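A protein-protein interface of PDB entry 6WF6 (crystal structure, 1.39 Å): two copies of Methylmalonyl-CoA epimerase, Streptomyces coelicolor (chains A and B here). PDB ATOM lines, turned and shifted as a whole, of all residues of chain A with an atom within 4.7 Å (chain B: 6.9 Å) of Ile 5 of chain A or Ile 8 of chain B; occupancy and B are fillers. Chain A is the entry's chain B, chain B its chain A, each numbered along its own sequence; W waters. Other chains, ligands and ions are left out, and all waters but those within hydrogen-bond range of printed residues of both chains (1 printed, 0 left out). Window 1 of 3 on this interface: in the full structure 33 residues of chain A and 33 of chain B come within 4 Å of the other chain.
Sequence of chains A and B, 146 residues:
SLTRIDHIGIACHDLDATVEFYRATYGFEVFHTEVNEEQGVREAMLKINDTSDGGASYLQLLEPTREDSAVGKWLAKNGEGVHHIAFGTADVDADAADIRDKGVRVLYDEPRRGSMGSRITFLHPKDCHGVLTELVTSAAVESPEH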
ATOM      1  N   ARG A   4       5.960  -6.372  16.902  1.00  0.00           N
ATOM      2  CA  ARG A   4       4.514  -6.136  16.668  1.00  0.00           C
ATOM      3  C   ARG A   4       4.272  -5.548  15.290  1.00  0.00           C
ATOM      4  O   ARG A   4       5.198  -4.959  14.717  1.00  0.00           O
ATOM      5  CB  ARG A   4       3.844  -5.231  17.699  1.00  0.00           C
ATOM      6  CG  ARG A   4       4.355  -3.802  17.680  1.00  0.00           C
ATOM      7  CD  ARG A   4       3.721  -2.875  18.695  1.00  0.00           C
ATOM      8  NE  ARG A   4       4.312  -1.548  18.600  1.00  0.00           N
ATOM      9  CZ  ARG A   4       5.485  -1.183  19.077  1.00  0.00           C
ATOM     10  NH1 ARG A   4       6.220  -2.015  19.795  1.00  0.00           N
ATOM     11  NH2 ARG A   4       5.926   0.028  18.791  1.00  0.00           N
ATOM     12  N   ILE A   5       3.020  -5.660  14.810  1.00  0.00           N
ATOM     13  CA  ILE A   5       2.497  -4.728  13.794  1.00  0.00           C
ATOM     14  C   ILE A   5       2.126  -3.460  14.548  1.00  0.00           C
ATOM     15  O   ILE A   5       1.273  -3.509  15.461  1.00  0.00           O
ATOM     16  CB  ILE A   5       1.330  -5.319  13.014  1.00  0.00           C
ATOM     17  CG1 ILE A   5       1.758  -6.555  12.217  1.00  0.00           C
ATOM     18  CG2 ILE A   5       0.693  -4.271  12.140  1.00  0.00           C
ATOM     19  CD1 ILE A   5       0.632  -7.389  11.682  1.00  0.00           C
ATOM     20  N   ASP A   6       2.810  -2.366  14.278  1.00  0.00           N
ATOM     21  CA  ASP A   6       2.557  -1.081  14.961  1.00  0.00           C
ATOM     22  C   ASP A   6       1.372  -0.368  14.290  1.00  0.00           C
ATOM     23  O   ASP A   6       0.480   0.119  14.994  1.00  0.00           O
ATOM     24  CB  ASP A   6       3.810  -0.191  14.966  1.00  0.00           C
ATOM     25  CG  ASP A   6       3.607   1.035  15.853  1.00  0.00           C
ATOM     26  OD1 ASP A   6       3.733   0.923  17.080  1.00  0.00           O
ATOM     27  OD2 ASP A   6       3.194   2.105  15.283  1.00  0.00           O
ATOM     28  N   HIS A   7       1.347  -0.287  12.976  1.00  0.00           N
ATOM     29  CA  HIS A   7       0.208   0.387  12.342  1.00  0.00           C
ATOM     30  C   HIS A   7       0.130   0.033  10.872  1.00  0.00           C
ATOM     31  O   HIS A   7       1.080  -0.466  10.233  1.00  0.00           O
ATOM     32  CB  HIS A   7       0.228   1.906  12.571  1.00  0.00           C
ATOM     33  CG  HIS A   7       1.376   2.670  12.006  1.00  0.00           C
ATOM     34  ND1 HIS A   7       2.496   2.912  12.769  1.00  0.00           N
ATOM     35  CD2 HIS A   7       1.538   3.309  10.831  1.00  0.00           C
ATOM     36  CE1 HIS A   7       3.313   3.667  12.027  1.00  0.00           C
ATOM     37  NE2 HIS A   7       2.765   3.955  10.831  1.00  0.00           N
ATOM     38  N   ILE A   8      -1.032   0.347  10.316  1.00  0.00           N
ATOM     39  CA  ILE A   8      -1.266   0.351   8.847  1.00  0.00           C
ATOM     40  C   ILE A   8      -1.365   1.817   8.433  1.00  0.00           C
ATOM     41  O   ILE A   8      -2.224   2.498   8.988  1.00  0.00           O
ATOM     42  CB  ILE A   8      -2.529  -0.474   8.500  1.00  0.00           C
ATOM     43  CG1 ILE A   8      -2.430  -1.905   9.048  1.00  0.00           C
ATOM     44  CG2 ILE A   8      -2.691  -0.446   7.000  1.00  0.00           C
ATOM     45  CD1 ILE A   8      -3.743  -2.656   8.988  1.00  0.00           C
ATOM     46  N   THR A  51      -0.933  -4.734  22.257  1.00  0.00           N
ATOM     47  CA  THR A  51      -0.108  -5.861  21.780  1.00  0.00           C
ATOM     48  C   THR A  51       0.731  -6.475  22.898  1.00  0.00           C
ATOM     49  O   THR A  51       1.044  -5.798  23.889  1.00  0.00           O
ATOM     50  CB  THR A  51       0.749  -5.419  20.574  1.00  0.00           C
ATOM     51  OG1 THR A  51       1.633  -4.370  20.982  1.00  0.00           O
ATOM     52  CG2 THR A  51      -0.067  -4.881  19.434  1.00  0.00           C
ATOM     53  N   ALA A  56       1.009  -1.098  20.987  1.00  0.00           N
ATOM     54  CA  ALA A  56      -0.368  -0.976  20.497  1.00  0.00           C
ATOM     55  C   ALA A  56      -0.316  -1.042  18.986  1.00  0.00           C
ATOM     56  O   ALA A  56       0.777  -0.912  18.385  1.00  0.00           O
ATOM     57  CB  ALA A  56      -1.050   0.304  20.958  1.00  0.00           C
ATOM     58  N   SER A  57      -1.460  -1.321  18.398  1.00  0.00           N
ATOM     59  CA  SER A  57      -1.608  -1.343  16.938  1.00  0.00           C
ATOM     60  C   SER A  57      -2.655  -0.306  16.534  1.00  0.00           C
ATOM     61  O   SER A  57      -3.750  -0.246  17.161  1.00  0.00           O
ATOM     62  CB  SER A  57      -2.033  -2.683  16.391  1.00  0.00           C
ATOM     63  OG  SER A  57      -1.089  -3.681  16.655  1.00  0.00           O
ATOM     64  N   ILE A  85       2.972  -0.347   5.702  1.00  0.00           N
ATOM     65  CA  ILE A  85       2.777  -1.110   6.960  1.00  0.00           C
ATOM     66  C   ILE A  85       3.914  -0.786   7.895  1.00  0.00           C
ATOM     67  O   ILE A  85       5.031  -0.475   7.375  1.00  0.00           O
ATOM     68  CB  ILE A  85       2.640  -2.604   6.669  1.00  0.00           C
ATOM     69  CG1 ILE A  85       3.927  -3.257   6.236  1.00  0.00           C
ATOM     70  CG2 ILE A  85       1.533  -2.835   5.628  1.00  0.00           C
ATOM     71  CD1 ILE A  85       3.830  -4.770   6.166  1.00  0.00           C
ATOM     72  N   ALA A  86       3.725  -0.814   9.186  1.00  0.00           N
ATOM     73  CA  ALA A  86       4.768  -0.419  10.138  1.00  0.00           C
ATOM     74  C   ALA A  86       4.905  -1.514  11.174  1.00  0.00           C
ATOM     75  O   ALA A  86       3.891  -1.972  11.759  1.00  0.00           O
ATOM     76  CB  ALA A  86       4.415   0.863  10.813  1.00  0.00           C
ATOM     77  N   PHE A  87       6.131  -1.864  11.511  1.00  0.00           N
ATOM     78  CA  PHE A  87       6.497  -2.840  12.556  1.00  0.00           C
ATOM     79  C   PHE A  87       7.152  -2.113  13.722  1.00  0.00           C
ATOM     80  O   PHE A  87       7.933  -1.194  13.449  1.00  0.00           O
ATOM     81  CB  PHE A  87       7.440  -3.891  11.994  1.00  0.00           C
ATOM     82  CG  PHE A  87       6.858  -4.769  10.924  1.00  0.00           C
ATOM     83  CD1 PHE A  87       5.932  -5.746  11.230  1.00  0.00           C
ATOM     84  CD2 PHE A  87       7.239  -4.587   9.613  1.00  0.00           C
ATOM     85  CE1 PHE A  87       5.376  -6.522  10.225  1.00  0.00           C
ATOM     86  CE2 PHE A  87       6.675  -5.370   8.609  1.00  0.00           C
ATOM     87  CZ  PHE A  87       5.765  -6.338   8.917  1.00  0.00           C
ATOM     88  N   ILE B   5      -6.664  -5.553  14.867  1.00  0.00           N
ATOM     89  CA  ILE B   5      -6.128  -5.842  13.514  1.00  0.00           C
ATOM     90  C   ILE B   5      -5.742  -7.316  13.524  1.00  0.00           C
ATOM     91  O   ILE B   5      -4.814  -7.717  14.261  1.00  0.00           O
ATOM     92  CB  ILE B   5      -4.947  -4.931  13.124  1.00  0.00           C
ATOM     93  CG1 ILE B   5      -5.401  -3.465  13.086  1.00  0.00           C
ATOM     94  CG2 ILE B   5      -4.290  -5.428  11.827  1.00  0.00           C
ATOM     95  CD1 ILE B   5      -4.309  -2.408  12.969  1.00  0.00           C
ATOM     96  N   ASP B   6      -6.478  -8.117  12.788  1.00  0.00           N
ATOM     97  CA  ASP B   6      -6.211  -9.558  12.686  1.00  0.00           C
ATOM     98  C   ASP B   6      -5.069  -9.841  11.737  1.00  0.00           C
ATOM     99  O   ASP B   6      -4.135 -10.613  12.132  1.00  0.00           O
ATOM    100  CB  ASP B   6      -7.426 -10.356  12.264  1.00  0.00           C
ATOM    101  CG  ASP B   6      -7.223 -11.859  12.428  1.00  0.00           C
ATOM    102  OD1 ASP B   6      -7.404 -12.342  13.596  1.00  0.00           O
ATOM    103  OD2 ASP B   6      -6.833 -12.512  11.444  1.00  0.00           O
ATOM    104  N   HIS B   7      -5.047  -9.250  10.553  1.00  0.00           N
ATOM    105  CA  HIS B   7      -3.906  -9.526   9.656  1.00  0.00           C
ATOM    106  C   HIS B   7      -3.845  -8.475   8.574  1.00  0.00           C
ATOM    107  O   HIS B   7      -4.838  -7.749   8.331  1.00  0.00           O
ATOM    108  CB  HIS B   7      -3.917 -10.963   9.120  1.00  0.00           C
ATOM    109  CG  HIS B   7      -5.107 -11.329   8.264  1.00  0.00           C
ATOM    110  ND1 HIS B   7      -6.219 -11.959   8.792  1.00  0.00           N
ATOM    111  CD2 HIS B   7      -5.300 -11.277   6.928  1.00  0.00           C
ATOM    112  CE1 HIS B   7      -7.037 -12.253   7.761  1.00  0.00           C
ATOM    113  NE2 HIS B   7      -6.556 -11.814   6.622  1.00  0.00           N
ATOM    114  N   ILE B   8      -2.702  -8.471   7.898  1.00  0.00           N
ATOM    115  CA  ILE B   8      -2.501  -7.718   6.643  1.00  0.00           C
ATOM    116  C   ILE B   8      -2.362  -8.774   5.566  1.00  0.00           C
ATOM    117  O   ILE B   8      -1.435  -9.609   5.688  1.00  0.00           O
ATOM    118  CB  ILE B   8      -1.265  -6.824   6.759  1.00  0.00           C
ATOM    119  CG1 ILE B   8      -1.347  -5.871   7.962  1.00  0.00           C
ATOM    120  CG2 ILE B   8      -1.085  -6.091   5.433  1.00  0.00           C
ATOM    121  CD1 ILE B   8      -0.035  -5.227   8.369  1.00  0.00           C
ATOM    122  N   GLY B   9      -3.164  -8.711   4.514  1.00  0.00           N
ATOM    123  CA  GLY B   9      -3.071  -9.609   3.358  1.00  0.00           C
ATOM    124  C   GLY B   9      -2.144  -9.041   2.311  1.00  0.00           C
ATOM    125  O   GLY B   9      -2.343  -7.907   1.868  1.00  0.00           O
ATOM    126  N   ILE B  10      -1.090  -9.764   2.005  1.00  0.00           N
ATOM    127  CA  ILE B  10       0.012  -9.339   1.110  1.00  0.00           C
ATOM    128  C   ILE B  10       0.043 -10.338  -0.039  1.00  0.00           C
ATOM    129  O   ILE B  10       0.281 -11.539   0.196  1.00  0.00           O
ATOM    130  CB  ILE B  10       1.317  -9.271   1.896  1.00  0.00           C
ATOM    131  CG1 ILE B  10       1.245  -8.220   2.993  1.00  0.00           C
ATOM    132  CG2 ILE B  10       2.487  -9.003   0.951  1.00  0.00           C
ATOM    133  CD1 ILE B  10       2.414  -8.144   3.871  1.00  0.00           C
ATOM    134  N   MET B  45       0.403 -17.774   6.964  1.00  0.00           N
ATOM    135  CA  MET B  45       0.244 -16.834   8.091  1.00  0.00           C
ATOM    136  C   MET B  45       1.555 -16.769   8.857  1.00  0.00           C
ATOM    137  O   MET B  45       2.072 -17.836   9.235  1.00  0.00           O
ATOM    138  CB  MET B  45      -0.879 -17.339   8.994  1.00  0.00           C
ATOM    139  CG  MET B  45      -2.229 -17.209   8.335  1.00  0.00           C
ATOM    140  SD  MET B  45      -2.840 -15.500   8.254  1.00  0.00           S
ATOM    141  CE  MET B  45      -4.004 -15.460   9.615  1.00  0.00           C
ATOM    142  N   LEU B  46       2.078 -15.569   9.093  1.00  0.00           N
ATOM    143  CA  LEU B  46       3.286 -15.322   9.917  1.00  0.00           C
ATOM    144  C   LEU B  46       2.769 -14.573  11.137  1.00  0.00           C
ATOM    145  O   LEU B  46       2.227 -13.447  10.990  1.00  0.00           O
ATOM    146  CB  LEU B  46       4.268 -14.474   9.117  1.00  0.00           C
ATOM    147  CG  LEU B  46       5.121 -15.139   8.040  1.00  0.00           C
ATOM    148  CD1 LEU B  46       4.393 -16.054   7.089  1.00  0.00           C
ATOM    149  CD2 LEU B  46       5.911 -14.061   7.285  1.00  0.00           C
ATOM    150  N   ILE B  48       2.942 -12.199  14.186  1.00  0.00           N
ATOM    151  CA  ILE B  48       3.838 -11.112  14.612  1.00  0.00           C
ATOM    152  C   ILE B  48       3.660 -10.867  16.093  1.00  0.00           C
ATOM    153  O   ILE B  48       4.679 -10.541  16.780  1.00  0.00           O
ATOM    154  CB  ILE B  48       3.625  -9.852  13.763  1.00  0.00           C
ATOM    155  CG1 ILE B  48       3.587 -10.193  12.273  1.00  0.00           C
ATOM    156  CG2 ILE B  48       4.732  -8.867  14.073  1.00  0.00           C
ATOM    157  CD1 ILE B  48       4.771 -10.957  11.749  1.00  0.00           C
ATOM    158  N   ASN B  49       2.461 -10.900  16.636  1.00  0.00           N
ATOM    159  CA  ASN B  49       2.238 -10.620  18.056  1.00  0.00           C
ATOM    160  C   ASN B  49       0.862 -11.181  18.456  1.00  0.00           C
ATOM    161  O   ASN B  49       0.027 -11.505  17.598  1.00  0.00           O
ATOM    162  CB  ASN B  49       2.364  -9.122  18.333  1.00  0.00           C
ATOM    163  CG  ASN B  49       1.412  -8.285  17.520  1.00  0.00           C
ATOM    164  OD1 ASN B  49       1.761  -7.850  16.402  1.00  0.00           O
ATOM    165  ND2 ASN B  49       0.216  -7.997  18.055  1.00  0.00           N
ATOM    166  N   SER B  57      -2.149 -11.036  15.671  1.00  0.00           N
ATOM    167  CA  SER B  57      -1.943 -10.265  14.453  1.00  0.00           C
ATOM    168  C   SER B  57      -0.938 -11.009  13.597  1.00  0.00           C
ATOM    169  O   SER B  57       0.177 -11.366  14.067  1.00  0.00           O
ATOM    170  CB  SER B  57      -1.499  -8.848  14.680  1.00  0.00           C
ATOM    171  OG  SER B  57      -2.487  -8.116  15.373  1.00  0.00           O
ATOM    172  N   TYR B  58      -1.258 -11.153  12.346  1.00  0.00           N
ATOM    173  CA  TYR B  58      -0.469 -11.898  11.364  1.00  0.00           C
ATOM    174  C   TYR B  58      -0.188 -11.055  10.121  1.00  0.00           C
ATOM    175  O   TYR B  58      -0.943 -10.155   9.766  1.00  0.00           O
ATOM    176  CB  TYR B  58      -1.192 -13.172  10.929  1.00  0.00           C
ATOM    177  CG  TYR B  58      -1.710 -14.104  12.000  1.00  0.00           C
ATOM    178  CD1 TYR B  58      -2.950 -13.867  12.587  1.00  0.00           C
ATOM    179  CD2 TYR B  58      -0.964 -15.188  12.424  1.00  0.00           C
ATOM    180  CE1 TYR B  58      -3.473 -14.740  13.543  1.00  0.00           C
ATOM    181  CE2 TYR B  58      -1.471 -16.039  13.389  1.00  0.00           C
ATOM    182  CZ  TYR B  58      -2.723 -15.836  13.919  1.00  0.00           C
ATOM    183  OH  TYR B  58      -3.186 -16.745  14.828  1.00  0.00           O
ATOM    184  N   LEU B  59       0.844 -11.462   9.403  1.00  0.00           N
ATOM    185  CA  LEU B  59       0.966 -11.199   7.955  1.00  0.00           C
ATOM    186  C   LEU B  59       0.429 -12.415   7.231  1.00  0.00           C
ATOM    187  O   LEU B  59       0.841 -13.555   7.551  1.00  0.00           O
ATOM    188  CB  LEU B  59       2.416 -10.973   7.525  1.00  0.00           C
ATOM    189  CG  LEU B  59       3.111  -9.845   8.276  1.00  0.00           C
ATOM    190  CD1 LEU B  59       4.571  -9.837   7.794  1.00  0.00           C
ATOM    191  CD2 LEU B  59       2.419  -8.490   8.049  1.00  0.00           C
ATOM    192  N   GLN B  60      -0.517 -12.223   6.323  1.00  0.00           N
ATOM    193  CA  GLN B  60      -1.113 -13.303   5.528  1.00  0.00           C
ATOM    194  C   GLN B  60      -0.564 -13.126   4.111  1.00  0.00           C
ATOM    195  O   GLN B  60      -1.018 -12.238   3.376  1.00  0.00           O
ATOM    196  CB  GLN B  60      -2.636 -13.192   5.548  1.00  0.00           C
ATOM    197  CG  GLN B  60      -3.318 -14.384   4.910  1.00  0.00           C
ATOM    198  CD  GLN B  60      -4.803 -14.157   4.969  1.00  0.00           C
ATOM    199  OE1 GLN B  60      -5.366 -13.247   4.332  1.00  0.00           O
ATOM    200  NE2 GLN B  60      -5.430 -14.932   5.823  1.00  0.00           N
ATOM    201  N   LEU B  61       0.426 -13.935   3.761  1.00  0.00           N
ATOM    202  CA  LEU B  61       1.065 -13.898   2.424  1.00  0.00           C
ATOM    203  C   LEU B  61       0.268 -14.817   1.513  1.00  0.00           C
ATOM    204  O   LEU B  61      -0.098 -15.943   1.944  1.00  0.00           O
ATOM    205  CB  LEU B  61       2.527 -14.331   2.516  1.00  0.00           C
ATOM    206  CG  LEU B  61       3.504 -13.215   2.865  1.00  0.00           C
ATOM    207  CD1 LEU B  61       3.139 -12.483   4.163  1.00  0.00           C
ATOM    208  CD2 LEU B  61       4.909 -13.793   2.949  1.00  0.00           C
ATOM    209  N   LEU B  62      -0.096 -14.369   0.338  1.00  0.00           N
ATOM    210  CA  LEU B  62      -1.066 -15.066  -0.532  1.00  0.00           C
ATOM    211  C   LEU B  62      -0.446 -15.193  -1.920  1.00  0.00           C
ATOM    212  O   LEU B  62      -0.027 -14.125  -2.452  1.00  0.00           O
ATOM    213  CB  LEU B  62      -2.332 -14.205  -0.742  1.00  0.00           C
ATOM    214  CG  LEU B  62      -3.408 -14.058   0.316  1.00  0.00           C
ATOM    215  CD1 LEU B  62      -3.428 -15.238   1.247  1.00  0.00           C
ATOM    216  CD2 LEU B  62      -3.333 -12.698   0.982  1.00  0.00           C
ATOM    217  N   VAL B  82       0.335  -4.904  -0.747  1.00  0.00           N
ATOM    218  CA  VAL B  82      -0.791  -5.082   0.200  1.00  0.00           C
ATOM    219  C   VAL B  82      -2.083  -5.213  -0.572  1.00  0.00           C
ATOM    220  O   VAL B  82      -2.432  -4.310  -1.339  1.00  0.00           O
ATOM    221  CB  VAL B  82      -0.876  -3.952   1.216  1.00  0.00           C
ATOM    222  CG1 VAL B  82      -2.086  -4.189   2.090  1.00  0.00           C
ATOM    223  CG2 VAL B  82       0.412  -3.865   2.017  1.00  0.00           C
ATOM    224  N   HIS B  83      -2.804  -6.286  -0.322  1.00  0.00           N
ATOM    225  CA  HIS B  83      -4.062  -6.628  -1.009  1.00  0.00           C
ATOM    226  C   HIS B  83      -5.270  -6.293  -0.137  1.00  0.00           C
ATOM    227  O   HIS B  83      -6.301  -5.788  -0.695  1.00  0.00           O
ATOM    228  CB  HIS B  83      -4.019  -8.119  -1.390  1.00  0.00           C
ATOM    229  CG  HIS B  83      -5.279  -8.651  -1.970  1.00  0.00           C
ATOM    230  ND1 HIS B  83      -6.199  -9.344  -1.222  1.00  0.00           N
ATOM    231  CD2 HIS B  83      -5.789  -8.561  -3.214  1.00  0.00           C
ATOM    232  CE1 HIS B  83      -7.222  -9.663  -1.994  1.00  0.00           C
ATOM    233  NE2 HIS B  83      -7.025  -9.174  -3.223  1.00  0.00           N
ATOM    234  N   HIS B  84      -5.202  -6.511   1.169  1.00  0.00           N
ATOM    235  CA  HIS B  84      -6.360  -6.220   2.048  1.00  0.00           C
ATOM    236  C   HIS B  84      -5.913  -6.085   3.477  1.00  0.00           C
ATOM    237  O   HIS B  84      -4.776  -6.490   3.790  1.00  0.00           O
ATOM    238  CB  HIS B  84      -7.420  -7.322   1.960  1.00  0.00           C
ATOM    239  CG  HIS B  84      -7.076  -8.706   2.429  1.00  0.00           C
ATOM    240  ND1 HIS B  84      -6.502  -9.663   1.591  1.00  0.00           N
ATOM    241  CD2 HIS B  84      -7.250  -9.346   3.613  1.00  0.00           C
ATOM    242  CE1 HIS B  84      -6.385 -10.817   2.270  1.00  0.00           C
ATOM    243  NE2 HIS B  84      -6.827 -10.669   3.502  1.00  0.00           N
ATOM    244  N   ILE B  85      -6.771  -5.594   4.335  1.00  0.00           N
ATOM    245  CA  ILE B  85      -6.548  -5.562   5.799  1.00  0.00           C
ATOM    246  C   ILE B  85      -7.707  -6.287   6.450  1.00  0.00           C
ATOM    247  O   ILE B  85      -8.812  -6.276   5.897  1.00  0.00           O
ATOM    248  CB  ILE B  85      -6.358  -4.132   6.321  1.00  0.00           C
ATOM    249  CG1 ILE B  85      -7.618  -3.322   6.273  1.00  0.00           C
ATOM    250  CG2 ILE B  85      -5.299  -3.412   5.527  1.00  0.00           C
ATOM    251  CD1 ILE B  85      -7.437  -1.913   6.852  1.00  0.00           C
ATOM    252  N   ALA B  86      -7.479  -6.883   7.571  1.00  0.00           N
ATOM    253  CA  ALA B  86      -8.490  -7.703   8.269  1.00  0.00           C
ATOM    254  C   ALA B  86      -8.625  -7.272   9.695  1.00  0.00           C
ATOM    255  O   ALA B  86      -7.620  -7.218  10.397  1.00  0.00           O
ATOM    256  CB  ALA B  86      -8.167  -9.194   8.165  1.00  0.00           C
HETATM  257  O   HOH W   1      -1.763  -6.146  16.937  1.00  0.00           O
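Water W1 lies within hydrogen-bond range of OG of Ser 57 of chain A (2.6 Å), OG of Ser 57 of chain B (2.6 Å) and ND2 of Asn 49 of chain B (2.9 Å).
Ile 5 of chain A touches five residues of chain B. Of chain A, only Ile 5 (3.96 Å) and Ile 85 (3.96 Å) come within 4 Å of Ile 8 of chain B. Of the printed residues of chain B, Ile 8 of chain A touches Ile 85. Of the printed residues of chain A, Ile 48 of chain B touches Arg 4 and Ile 5. Of the printed residues of chain B, Thr 51 of chain A touches Asn 49. Printed residues of chain A within 4 Å of Asn 49 of chain B: Arg 4 (3.3 Å), Ile 5 (3.0 Å) and Thr 51 (3.4 Å). The nearest printed residue of chain A that does not touch Ser 57 of chain B is Ser 57 of chain A (4.8 Å).
Ile 5 of chain A touches Ile 8 of chain B, but with the chains exchanged Ile 8 of chain A does not touch Ile 5 of chain B (4.01 Å). Ile 5 of chain A touches Ser 57 of chain B, but with the chains exchanged Ser 57 of chain A does not touch Ile 5 of chain B (4.1 Å). Ile 8 of chain A touches Ile 85 of chain B, and with the chains exchanged Ile 85 of chain A touches Ile 8 of chain B.
Among the printed residues, merely in contact across the chains: Arg 4 of chain A with Asn 49 of chain B (3.3 Å), Thr 51 of chain A with Asn 49 of chain B (3.4 Å), Arg 4 of chain A with Ile 48 of chain B (3.6 Å), Ile 5 of chain A with Ile 48 of chain B (3.7 Å), Ile 5 of chain A with Tyr 58 of chain B (3.7 Å), Phe 87 of chain A with Leu 59 of chain B (3.9 Å), Ile 8 of chain A with Ile 85 of chain B (3.9 Å), Ile 85 of chain A with Val 82 of chain B (3.9 Å), Ile 5 of chain A with Ser 57 of chain B (3.96 Å), Ile 5 of chain A with Ile 8 of chain B (3.96 Å) and Ile 85 of chain A with Ile 8 of chain B (3.96 Å).
The backbone NH (N) of Leu 46 of chain B is in hydrogen-bond range of the backbone carbonyl oxygen (O) of Leu 59 of chain B (2.8 Å). O of Ile 5 of chain B lies within hydrogen-bond range of OG of Ser 57 of chain B, 2.6 Å away. The side-chain carboxylate (OD1) of Asp 6 of chain A is in salt-bridge range of the guanidinium group (NH2) of Arg 4 of chain A, at 2.9 Å. The backbone carbonyl oxygen (O) of Tyr 58 of chain B sits at hydrogen-bond distance from the backbone NH (N) of Ile 8 of chain B, 3.1 Å away. The backbone carbonyl oxygen (O) of Ile 8 of chain B is in hydrogen-bond range of the backbone NH (N) of Gln 60 of chain B (2.8 Å). The side-chain hydroxyl of Thr 51 of chain A sits at hydrogen-bond distance from the backbone NH of Ala 56 of chain A, 3.3 Å away.
The side-chain amide oxygen (OD1) of Asn 49 of chain B sits at hydrogen-bond distance from the backbone NH (N) of Ile 5 of chain A, at 3.0 Å.
Hydrophobic or aromatic side chains of chain A that line the printed part of chain B: Ile 5, Ile 8, Ile 85 and Phe 87. Of the 21 printed residues of chain B, 8 touch a printed residue of chain A. Hydrophobic or aromatic side chains of chain B that line the printed part of chain A: Ile 8, Ile 48, Leu 59, Val 82 and Ile 85. Among the printed residues, 12 pairs touch across the chains. Among the printed residues, no Asp or Glu carboxylate lies within 4 Å of a Lys or Arg side-chain nitrogen of the other chain.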
